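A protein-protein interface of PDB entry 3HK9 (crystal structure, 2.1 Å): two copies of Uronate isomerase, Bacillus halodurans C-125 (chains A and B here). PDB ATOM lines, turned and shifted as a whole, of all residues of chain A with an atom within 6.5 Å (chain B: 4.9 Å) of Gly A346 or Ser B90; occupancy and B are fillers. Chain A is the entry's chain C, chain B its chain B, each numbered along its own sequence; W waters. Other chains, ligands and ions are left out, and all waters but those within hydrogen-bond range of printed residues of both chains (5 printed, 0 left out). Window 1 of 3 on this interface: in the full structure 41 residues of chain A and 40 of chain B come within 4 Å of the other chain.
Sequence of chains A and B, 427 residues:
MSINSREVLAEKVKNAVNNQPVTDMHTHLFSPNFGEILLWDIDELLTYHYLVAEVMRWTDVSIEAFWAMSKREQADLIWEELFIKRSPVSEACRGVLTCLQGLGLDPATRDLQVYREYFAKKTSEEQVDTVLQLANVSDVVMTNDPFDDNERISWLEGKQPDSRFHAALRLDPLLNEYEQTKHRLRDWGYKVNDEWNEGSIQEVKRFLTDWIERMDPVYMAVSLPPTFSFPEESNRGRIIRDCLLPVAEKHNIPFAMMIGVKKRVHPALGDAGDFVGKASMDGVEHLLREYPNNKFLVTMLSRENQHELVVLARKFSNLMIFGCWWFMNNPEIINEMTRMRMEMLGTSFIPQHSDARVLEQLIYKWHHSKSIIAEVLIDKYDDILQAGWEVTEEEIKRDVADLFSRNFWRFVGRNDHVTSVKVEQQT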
ATOM      1  N   ARG A 314      28.599  -8.557  -0.744  1.00  0.00           N
ATOM      2  CA  ARG A 314      28.999  -9.963  -0.693  1.00  0.00           C
ATOM      3  C   ARG A 314      30.212 -10.116   0.238  1.00  0.00           C
ATOM      4  O   ARG A 314      30.415 -11.170   0.847  1.00  0.00           O
ATOM      5  CB  ARG A 314      29.401 -10.480  -2.088  1.00  0.00           C
ATOM      6  CG  ARG A 314      28.260 -10.746  -3.056  1.00  0.00           C
ATOM      7  CD  ARG A 314      28.804 -11.246  -4.399  1.00  0.00           C
ATOM      8  NE  ARG A 314      29.542 -12.498  -4.256  1.00  0.00           N
ATOM      9  CZ  ARG A 314      28.981 -13.691  -4.076  1.00  0.00           C
ATOM     10  NH1 ARG A 314      27.656 -13.811  -4.024  1.00  0.00           N
ATOM     11  NH2 ARG A 314      29.746 -14.765  -3.934  1.00  0.00           N
ATOM     12  N   ARG A 341      21.228  -7.684  -7.650  1.00  0.00           N
ATOM     13  CA  ARG A 341      21.209  -7.931  -6.216  1.00  0.00           C
ATOM     14  C   ARG A 341      20.803  -9.366  -5.881  1.00  0.00           C
ATOM     15  O   ARG A 341      21.529 -10.061  -5.183  1.00  0.00           O
ATOM     16  CB  ARG A 341      20.261  -6.944  -5.524  1.00  0.00           C
ATOM     17  CG  ARG A 341      20.784  -5.533  -5.517  1.00  0.00           C
ATOM     18  CD  ARG A 341      19.745  -4.533  -5.060  1.00  0.00           C
ATOM     19  NE  ARG A 341      20.353  -3.234  -4.792  1.00  0.00           N
ATOM     20  CZ  ARG A 341      19.687  -2.185  -4.325  1.00  0.00           C
ATOM     21  NH1 ARG A 341      18.386  -2.280  -4.081  1.00  0.00           N
ATOM     22  NH2 ARG A 341      20.326  -1.049  -4.076  1.00  0.00           N
ATOM     23  N   MET A 342      19.658  -9.816  -6.391  1.00  0.00           N
ATOM     24  CA  MET A 342      19.184 -11.170  -6.103  1.00  0.00           C
ATOM     25  C   MET A 342      20.117 -12.256  -6.623  1.00  0.00           C
ATOM     26  O   MET A 342      20.279 -13.305  -5.990  1.00  0.00           O
ATOM     27  CB  MET A 342      17.778 -11.393  -6.679  1.00  0.00           C
ATOM     28  CG  MET A 342      17.161 -12.715  -6.239  1.00  0.00           C
ATOM     29  SD  MET A 342      15.353 -12.786  -6.428  1.00  0.00           S
ATOM     30  CE  MET A 342      14.852 -11.626  -5.165  1.00  0.00           C
ATOM     31  N   GLU A 343      20.728 -12.008  -7.775  1.00  0.00           N
ATOM     32  CA  GLU A 343      21.641 -12.973  -8.361  1.00  0.00           C
ATOM     33  C   GLU A 343      22.919 -13.157  -7.541  1.00  0.00           C
ATOM     34  O   GLU A 343      23.486 -14.252  -7.519  1.00  0.00           O
ATOM     35  CB  GLU A 343      21.955 -12.570  -9.814  1.00  0.00           C
ATOM     36  CG  GLU A 343      20.803 -12.949 -10.764  1.00  0.00           C
ATOM     37  CD  GLU A 343      20.882 -12.335 -12.150  1.00  0.00           C
ATOM     38  OE1 GLU A 343      21.954 -11.837 -12.552  1.00  0.00           O
ATOM     39  OE2 GLU A 343      19.850 -12.367 -12.849  1.00  0.00           O
ATOM     40  N   MET A 344      23.364 -12.105  -6.851  1.00  0.00           N
ATOM     41  CA  MET A 344      24.582 -12.198  -6.045  1.00  0.00           C
ATOM     42  C   MET A 344      24.352 -12.248  -4.529  1.00  0.00           C
ATOM     43  O   MET A 344      25.266 -12.583  -3.779  1.00  0.00           O
ATOM     44  CB  MET A 344      25.534 -11.033  -6.369  1.00  0.00           C
ATOM     45  CG  MET A 344      26.422 -11.245  -7.608  1.00  0.00           C
ATOM     46  SD  MET A 344      27.578  -9.865  -7.952  1.00  0.00           S
ATOM     47  CE  MET A 344      26.428  -8.731  -8.803  1.00  0.00           C
ATOM     48  N   LEU A 345      23.137 -11.932  -4.079  1.00  0.00           N
ATOM     49  CA  LEU A 345      22.841 -11.929  -2.643  1.00  0.00           C
ATOM     50  C   LEU A 345      21.625 -12.759  -2.239  1.00  0.00           C
ATOM     51  O   LEU A 345      21.225 -12.741  -1.075  1.00  0.00           O
ATOM     52  CB  LEU A 345      22.607 -10.496  -2.166  1.00  0.00           C
ATOM     53  CG  LEU A 345      23.658  -9.442  -2.498  1.00  0.00           C
ATOM     54  CD1 LEU A 345      23.106  -8.068  -2.150  1.00  0.00           C
ATOM     55  CD2 LEU A 345      24.940  -9.734  -1.730  1.00  0.00           C
ATOM     56  N   GLY A 346      21.028 -13.480  -3.181  1.00  0.00           N
ATOM     57  CA  GLY A 346      19.852 -14.254  -2.837  1.00  0.00           C
ATOM     58  C   GLY A 346      18.807 -13.283  -2.307  1.00  0.00           C
ATOM     59  O   GLY A 346      18.448 -12.325  -2.989  1.00  0.00           O
ATOM     60  N   THR A 347      18.323 -13.504  -1.089  1.00  0.00           N
ATOM     61  CA  THR A 347      17.321 -12.604  -0.519  1.00  0.00           C
ATOM     62  C   THR A 347      17.862 -11.733   0.615  1.00  0.00           C
ATOM     63  O   THR A 347      17.084 -11.115   1.338  1.00  0.00           O
ATOM     64  CB  THR A 347      16.103 -13.384   0.024  1.00  0.00           C
ATOM     65  OG1 THR A 347      16.543 -14.349   0.992  1.00  0.00           O
ATOM     66  CG2 THR A 347      15.368 -14.089  -1.108  1.00  0.00           C
ATOM     67  N   SER A 348      19.184 -11.663   0.756  1.00  0.00           N
ATOM     68  CA  SER A 348      19.787 -10.880   1.833  1.00  0.00           C
ATOM     69  C   SER A 348      19.995  -9.388   1.553  1.00  0.00           C
ATOM     70  O   SER A 348      21.105  -8.872   1.682  1.00  0.00           O
ATOM     71  CB  SER A 348      21.122 -11.514   2.263  1.00  0.00           C
ATOM     72  OG  SER A 348      22.068 -11.496   1.209  1.00  0.00           O
ATOM     73  N   PHE A 349      18.921  -8.700   1.172  1.00  0.00           N
ATOM     74  CA  PHE A 349      18.977  -7.268   0.917  1.00  0.00           C
ATOM     75  C   PHE A 349      17.567  -6.704   0.987  1.00  0.00           C
ATOM     76  O   PHE A 349      16.594  -7.466   1.054  1.00  0.00           O
ATOM     77  CB  PHE A 349      19.623  -6.971  -0.452  1.00  0.00           C
ATOM     78  CG  PHE A 349      18.748  -7.290  -1.636  1.00  0.00           C
ATOM     79  CD1 PHE A 349      17.985  -6.291  -2.243  1.00  0.00           C
ATOM     80  CD2 PHE A 349      18.698  -8.583  -2.154  1.00  0.00           C
ATOM     81  CE1 PHE A 349      17.178  -6.573  -3.357  1.00  0.00           C
ATOM     82  CE2 PHE A 349      17.896  -8.881  -3.267  1.00  0.00           C
ATOM     83  CZ  PHE A 349      17.136  -7.875  -3.867  1.00  0.00           C
ATOM     84  N   LYS A 380      13.342 -15.940 -10.952  1.00  0.00           N
ATOM     85  CA  LYS A 380      14.264 -16.666 -10.080  1.00  0.00           C
ATOM     86  C   LYS A 380      13.702 -17.977  -9.545  1.00  0.00           C
ATOM     87  O   LYS A 380      14.402 -18.988  -9.529  1.00  0.00           O
ATOM     88  CB  LYS A 380      14.732 -15.765  -8.932  1.00  0.00           C
ATOM     89  CG  LYS A 380      15.960 -14.920  -9.300  1.00  0.00           C
ATOM     90  CD  LYS A 380      15.676 -13.959 -10.461  1.00  0.00           C
ATOM     91  CE  LYS A 380      16.911 -13.140 -10.836  1.00  0.00           C
ATOM     92  NZ  LYS A 380      17.939 -13.943 -11.555  1.00  0.00           N
ATOM     93  N   ILE A 384      14.909 -22.105 -10.408  1.00  0.00           N
ATOM     94  CA  ILE A 384      15.228 -23.246  -9.561  1.00  0.00           C
ATOM     95  C   ILE A 384      14.178 -24.341  -9.696  1.00  0.00           C
ATOM     96  O   ILE A 384      14.459 -25.513  -9.459  1.00  0.00           O
ATOM     97  CB  ILE A 384      15.436 -22.838  -8.080  1.00  0.00           C
ATOM     98  CG1 ILE A 384      14.257 -22.023  -7.563  1.00  0.00           C
ATOM     99  CG2 ILE A 384      16.743 -22.052  -7.957  1.00  0.00           C
ATOM    100  CD1 ILE A 384      14.333 -21.759  -6.066  1.00  0.00           C
ATOM    101  N   LEU A 403      12.161  -9.714   2.266  1.00  0.00           N
ATOM    102  CA  LEU A 403      12.460  -8.604   1.364  1.00  0.00           C
ATOM    103  C   LEU A 403      11.744  -7.293   1.701  1.00  0.00           C
ATOM    104  O   LEU A 403      12.370  -6.234   1.748  1.00  0.00           O
ATOM    105  CB  LEU A 403      12.126  -9.010  -0.080  1.00  0.00           C
ATOM    106  CG  LEU A 403      12.981 -10.148  -0.654  1.00  0.00           C
ATOM    107  CD1 LEU A 403      12.426 -10.585  -2.005  1.00  0.00           C
ATOM    108  CD2 LEU A 403      14.434  -9.686  -0.789  1.00  0.00           C
ATOM    109  N   GLU B  54      28.108 -15.752   0.602  1.00  0.00           N
ATOM    110  CA  GLU B  54      26.665 -15.673   0.778  1.00  0.00           C
ATOM    111  C   GLU B  54      26.155 -16.161   2.131  1.00  0.00           C
ATOM    112  O   GLU B  54      25.285 -15.530   2.728  1.00  0.00           O
ATOM    113  CB  GLU B  54      25.956 -16.416  -0.365  1.00  0.00           C
ATOM    114  CG  GLU B  54      26.023 -15.656  -1.693  1.00  0.00           C
ATOM    115  CD  GLU B  54      25.423 -16.419  -2.866  1.00  0.00           C
ATOM    116  OE1 GLU B  54      24.313 -16.978  -2.721  1.00  0.00           O
ATOM    117  OE2 GLU B  54      26.062 -16.445  -3.942  1.00  0.00           O
ATOM    118  N   PRO B  88      16.864 -20.996  -2.338  1.00  0.00           N
ATOM    119  CA  PRO B  88      18.162 -20.903  -3.017  1.00  0.00           C
ATOM    120  C   PRO B  88      18.059 -20.236  -4.389  1.00  0.00           C
ATOM    121  O   PRO B  88      18.385 -20.852  -5.400  1.00  0.00           O
ATOM    122  CB  PRO B  88      18.584 -22.359  -3.132  1.00  0.00           C
ATOM    123  CG  PRO B  88      17.269 -23.057  -3.359  1.00  0.00           C
ATOM    124  CD  PRO B  88      16.365 -22.385  -2.343  1.00  0.00           C
ATOM    125  N   VAL B  89      17.626 -18.981  -4.418  1.00  0.00           N
ATOM    126  CA  VAL B  89      17.453 -18.272  -5.684  1.00  0.00           C
ATOM    127  C   VAL B  89      18.670 -17.571  -6.285  1.00  0.00           C
ATOM    128  O   VAL B  89      18.639 -17.191  -7.457  1.00  0.00           O
ATOM    129  CB  VAL B  89      16.300 -17.243  -5.588  1.00  0.00           C
ATOM    130  CG1 VAL B  89      14.989 -17.967  -5.333  1.00  0.00           C
ATOM    131  CG2 VAL B  89      16.582 -16.230  -4.485  1.00  0.00           C
ATOM    132  N   SER B  90      19.738 -17.396  -5.511  1.00  0.00           N
ATOM    133  CA  SER B  90      20.926 -16.732  -6.045  1.00  0.00           C
ATOM    134  C   SER B  90      21.508 -17.600  -7.158  1.00  0.00           C
ATOM    135  O   SER B  90      21.247 -18.798  -7.211  1.00  0.00           O
ATOM    136  CB  SER B  90      21.973 -16.530  -4.949  1.00  0.00           C
ATOM    137  OG  SER B  90      22.574 -17.764  -4.604  1.00  0.00           O
ATOM    138  N   GLU B  91      22.303 -17.004  -8.039  1.00  0.00           N
ATOM    139  CA  GLU B  91      22.897 -17.752  -9.143  1.00  0.00           C
ATOM    140  C   GLU B  91      23.746 -18.920  -8.672  1.00  0.00           C
ATOM    141  O   GLU B  91      23.635 -20.024  -9.213  1.00  0.00           O
ATOM    142  CB  GLU B  91      23.740 -16.827 -10.024  1.00  0.00           C
ATOM    143  CG  GLU B  91      24.560 -17.524 -11.114  1.00  0.00           C
ATOM    144  CD  GLU B  91      23.715 -18.295 -12.131  1.00  0.00           C
ATOM    145  OE1 GLU B  91      22.486 -18.084 -12.201  1.00  0.00           O
ATOM    146  OE2 GLU B  91      24.295 -19.110 -12.882  1.00  0.00           O
ATOM    147  N   ALA B  92      24.586 -18.686  -7.663  1.00  0.00           N
ATOM    148  CA  ALA B  92      25.461 -19.737  -7.140  1.00  0.00           C
ATOM    149  C   ALA B  92      24.686 -20.905  -6.536  1.00  0.00           C
ATOM    150  O   ALA B  92      25.056 -22.068  -6.727  1.00  0.00           O
ATOM    151  CB  ALA B  92      26.417 -19.155  -6.102  1.00  0.00           C
ATOM    152  N   CYS B  93      23.620 -20.600  -5.799  1.00  0.00           N
ATOM    153  CA  CYS B  93      22.799 -21.643  -5.186  1.00  0.00           C
ATOM    154  C   CYS B  93      22.000 -22.389  -6.254  1.00  0.00           C
ATOM    155  O   CYS B  93      21.777 -23.596  -6.143  1.00  0.00           O
ATOM    156  CB  CYS B  93      21.863 -21.032  -4.141  1.00  0.00           C
ATOM    157  SG  CYS B  93      22.764 -20.386  -2.704  1.00  0.00           S
ATOM    158  N   ARG B  94      21.574 -21.664  -7.287  1.00  0.00           N
ATOM    159  CA  ARG B  94      20.833 -22.257  -8.408  1.00  0.00           C
ATOM    160  C   ARG B  94      21.774 -23.236  -9.113  1.00  0.00           C
ATOM    161  O   ARG B  94      21.362 -24.314  -9.553  1.00  0.00           O
ATOM    162  CB  ARG B  94      20.405 -21.161  -9.394  1.00  0.00           C
ATOM    163  CG  ARG B  94      19.814 -21.655 -10.717  1.00  0.00           C
ATOM    164  CD  ARG B  94      19.935 -20.556 -11.785  1.00  0.00           C
ATOM    165  NE  ARG B  94      19.482 -20.979 -13.108  1.00  0.00           N
ATOM    166  CZ  ARG B  94      19.825 -20.371 -14.243  1.00  0.00           C
ATOM    167  NH1 ARG B  94      20.633 -19.318 -14.226  1.00  0.00           N
ATOM    168  NH2 ARG B  94      19.340 -20.804 -15.400  1.00  0.00           N
ATOM    169  N   GLY B  95      23.048 -22.855  -9.199  1.00  0.00           N
ATOM    170  CA  GLY B  95      24.041 -23.699  -9.847  1.00  0.00           C
ATOM    171  C   GLY B  95      24.223 -25.055  -9.185  1.00  0.00           C
ATOM    172  O   GLY B  95      24.338 -26.081  -9.857  1.00  0.00           O
HETATM  173  O   HOH W   1      17.234 -18.566  -9.381  1.00  0.00           O
HETATM  174  O   HOH W   2      23.601 -14.102   0.860  1.00  0.00           O
HETATM  175  O   HOH W   3      19.452 -15.247  -9.352  1.00  0.00           O
HETATM  176  O   HOH W   4      22.612 -15.743  -1.122  1.00  0.00           O
HETATM  177  O   HOH W   5      25.317 -16.116  -6.471  1.00  0.00           O
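The backbone carbonyl oxygen of Glu A343 is in hydrogen-bond range of the backbone NH of Glu B91, at 3.0 Å. OE2 of Glu B54 is in salt-bridge range of NH1 of Arg A314.
NH1 of Arg B94 lies within salt-bridge range of OE1 of Glu B91 (3.0 Å). The backbone carbonyl oxygen (O) of Met A344 sits at hydrogen-bond distance from the guanidinium group (NH1) of Arg A314. The side-chain hydroxyl (OG) of Ser B90 is in hydrogen-bond range of the side-chain carboxylate (OE1) of Glu B54 (2.7 Å). OE2 of Glu A343 lies within salt-bridge range of NZ of Lys A380 (2.8 Å). The side-chain hydroxyl (OG) of Ser B90 is in hydrogen-bond range of the side-chain sulfur (SG) of Cys B93 (3.2 Å). OE1 of Glu B54 lies within hydrogen-bond range of SG of Cys B93 (3.7 Å).
Met A342 touches Val B89 (CG to CG2, 3.97 Å). Met A342 touches Ser B90. Glu A343 touches Ser B90 (O to CB, 3.8 Å). CG of Glu B54 touches O of Met A344, 3.8 Å away. N of Gly A346 touches CB of Ser B90 (3.6 Å). Lys A380 touches Val B89. O of Pro B88 touches CG2 of Ile A384, at 3.3 Å. Ile A384 touches Val B89.
Of the printed residues of chain B, Gly A346 touches Ser B90 (3.6 Å). Ser B90 touches just these residues of chain A: Met A342, Glu A343 and Gly A346. Of the printed residues of chain B, Met A342 touches Val B89 and Ser B90. Of the printed residues of chain B, Arg A314 touches Glu B54. Of the printed residues of chain B, Lys A380 touches Val B89. Of the printed residues of chain B, Ile A384 touches Pro B88 (3.3 Å) and Val B89 (3.9 Å). Phe A349 touches none of the printed residues of chain B. The nearest residue of chain B that does not touch Gly A346 is Val B89 (4.2 Å).
Printed residues of chain A that touch a printed residue of chain B: Arg A314, Met A342, Glu A343, Met A344, Gly A346, Lys A380 and Ile A384. Hydrophobic or aromatic side chains of chain A that line the printed part of chain B: Met A342 and Ile A384. Along chain A the printed residues that touch a printed residue of chain B span positions 314 to 384. Of the 9 printed residues of chain B, 5 touch a printed residue of chain A. Along chain B the printed residues that touch a printed residue of chain A span positions 54 to 91. Among the printed residues, 10 pairs touch across the chains.
No position is printed for both chains.
Water W4 lies within hydrogen-bond range of OE1 of Glu B54 (2.6 Å), O of Leu A345 (3.3 Å) and N of Gly A346 (3.4 Å). Water W5 lies within hydrogen-bond range of the side-chain carboxylate (OE2) of Glu B54, the backbone carbonyl oxygen (O) of Glu A343 and the backbone NH (N) of Ala B92. Water W1 bridges O of Val B89 (2.8 Å) and O of Lys A380 (2.9 Å). Water W3 bridges O of Val B89 and NZ of Lys A380. Water W2 lies within hydrogen-bond range of O of Glu B54 (2.9 Å), OG of Ser A348 (3.0 Å) and O of Leu A345 (3.4 Å).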
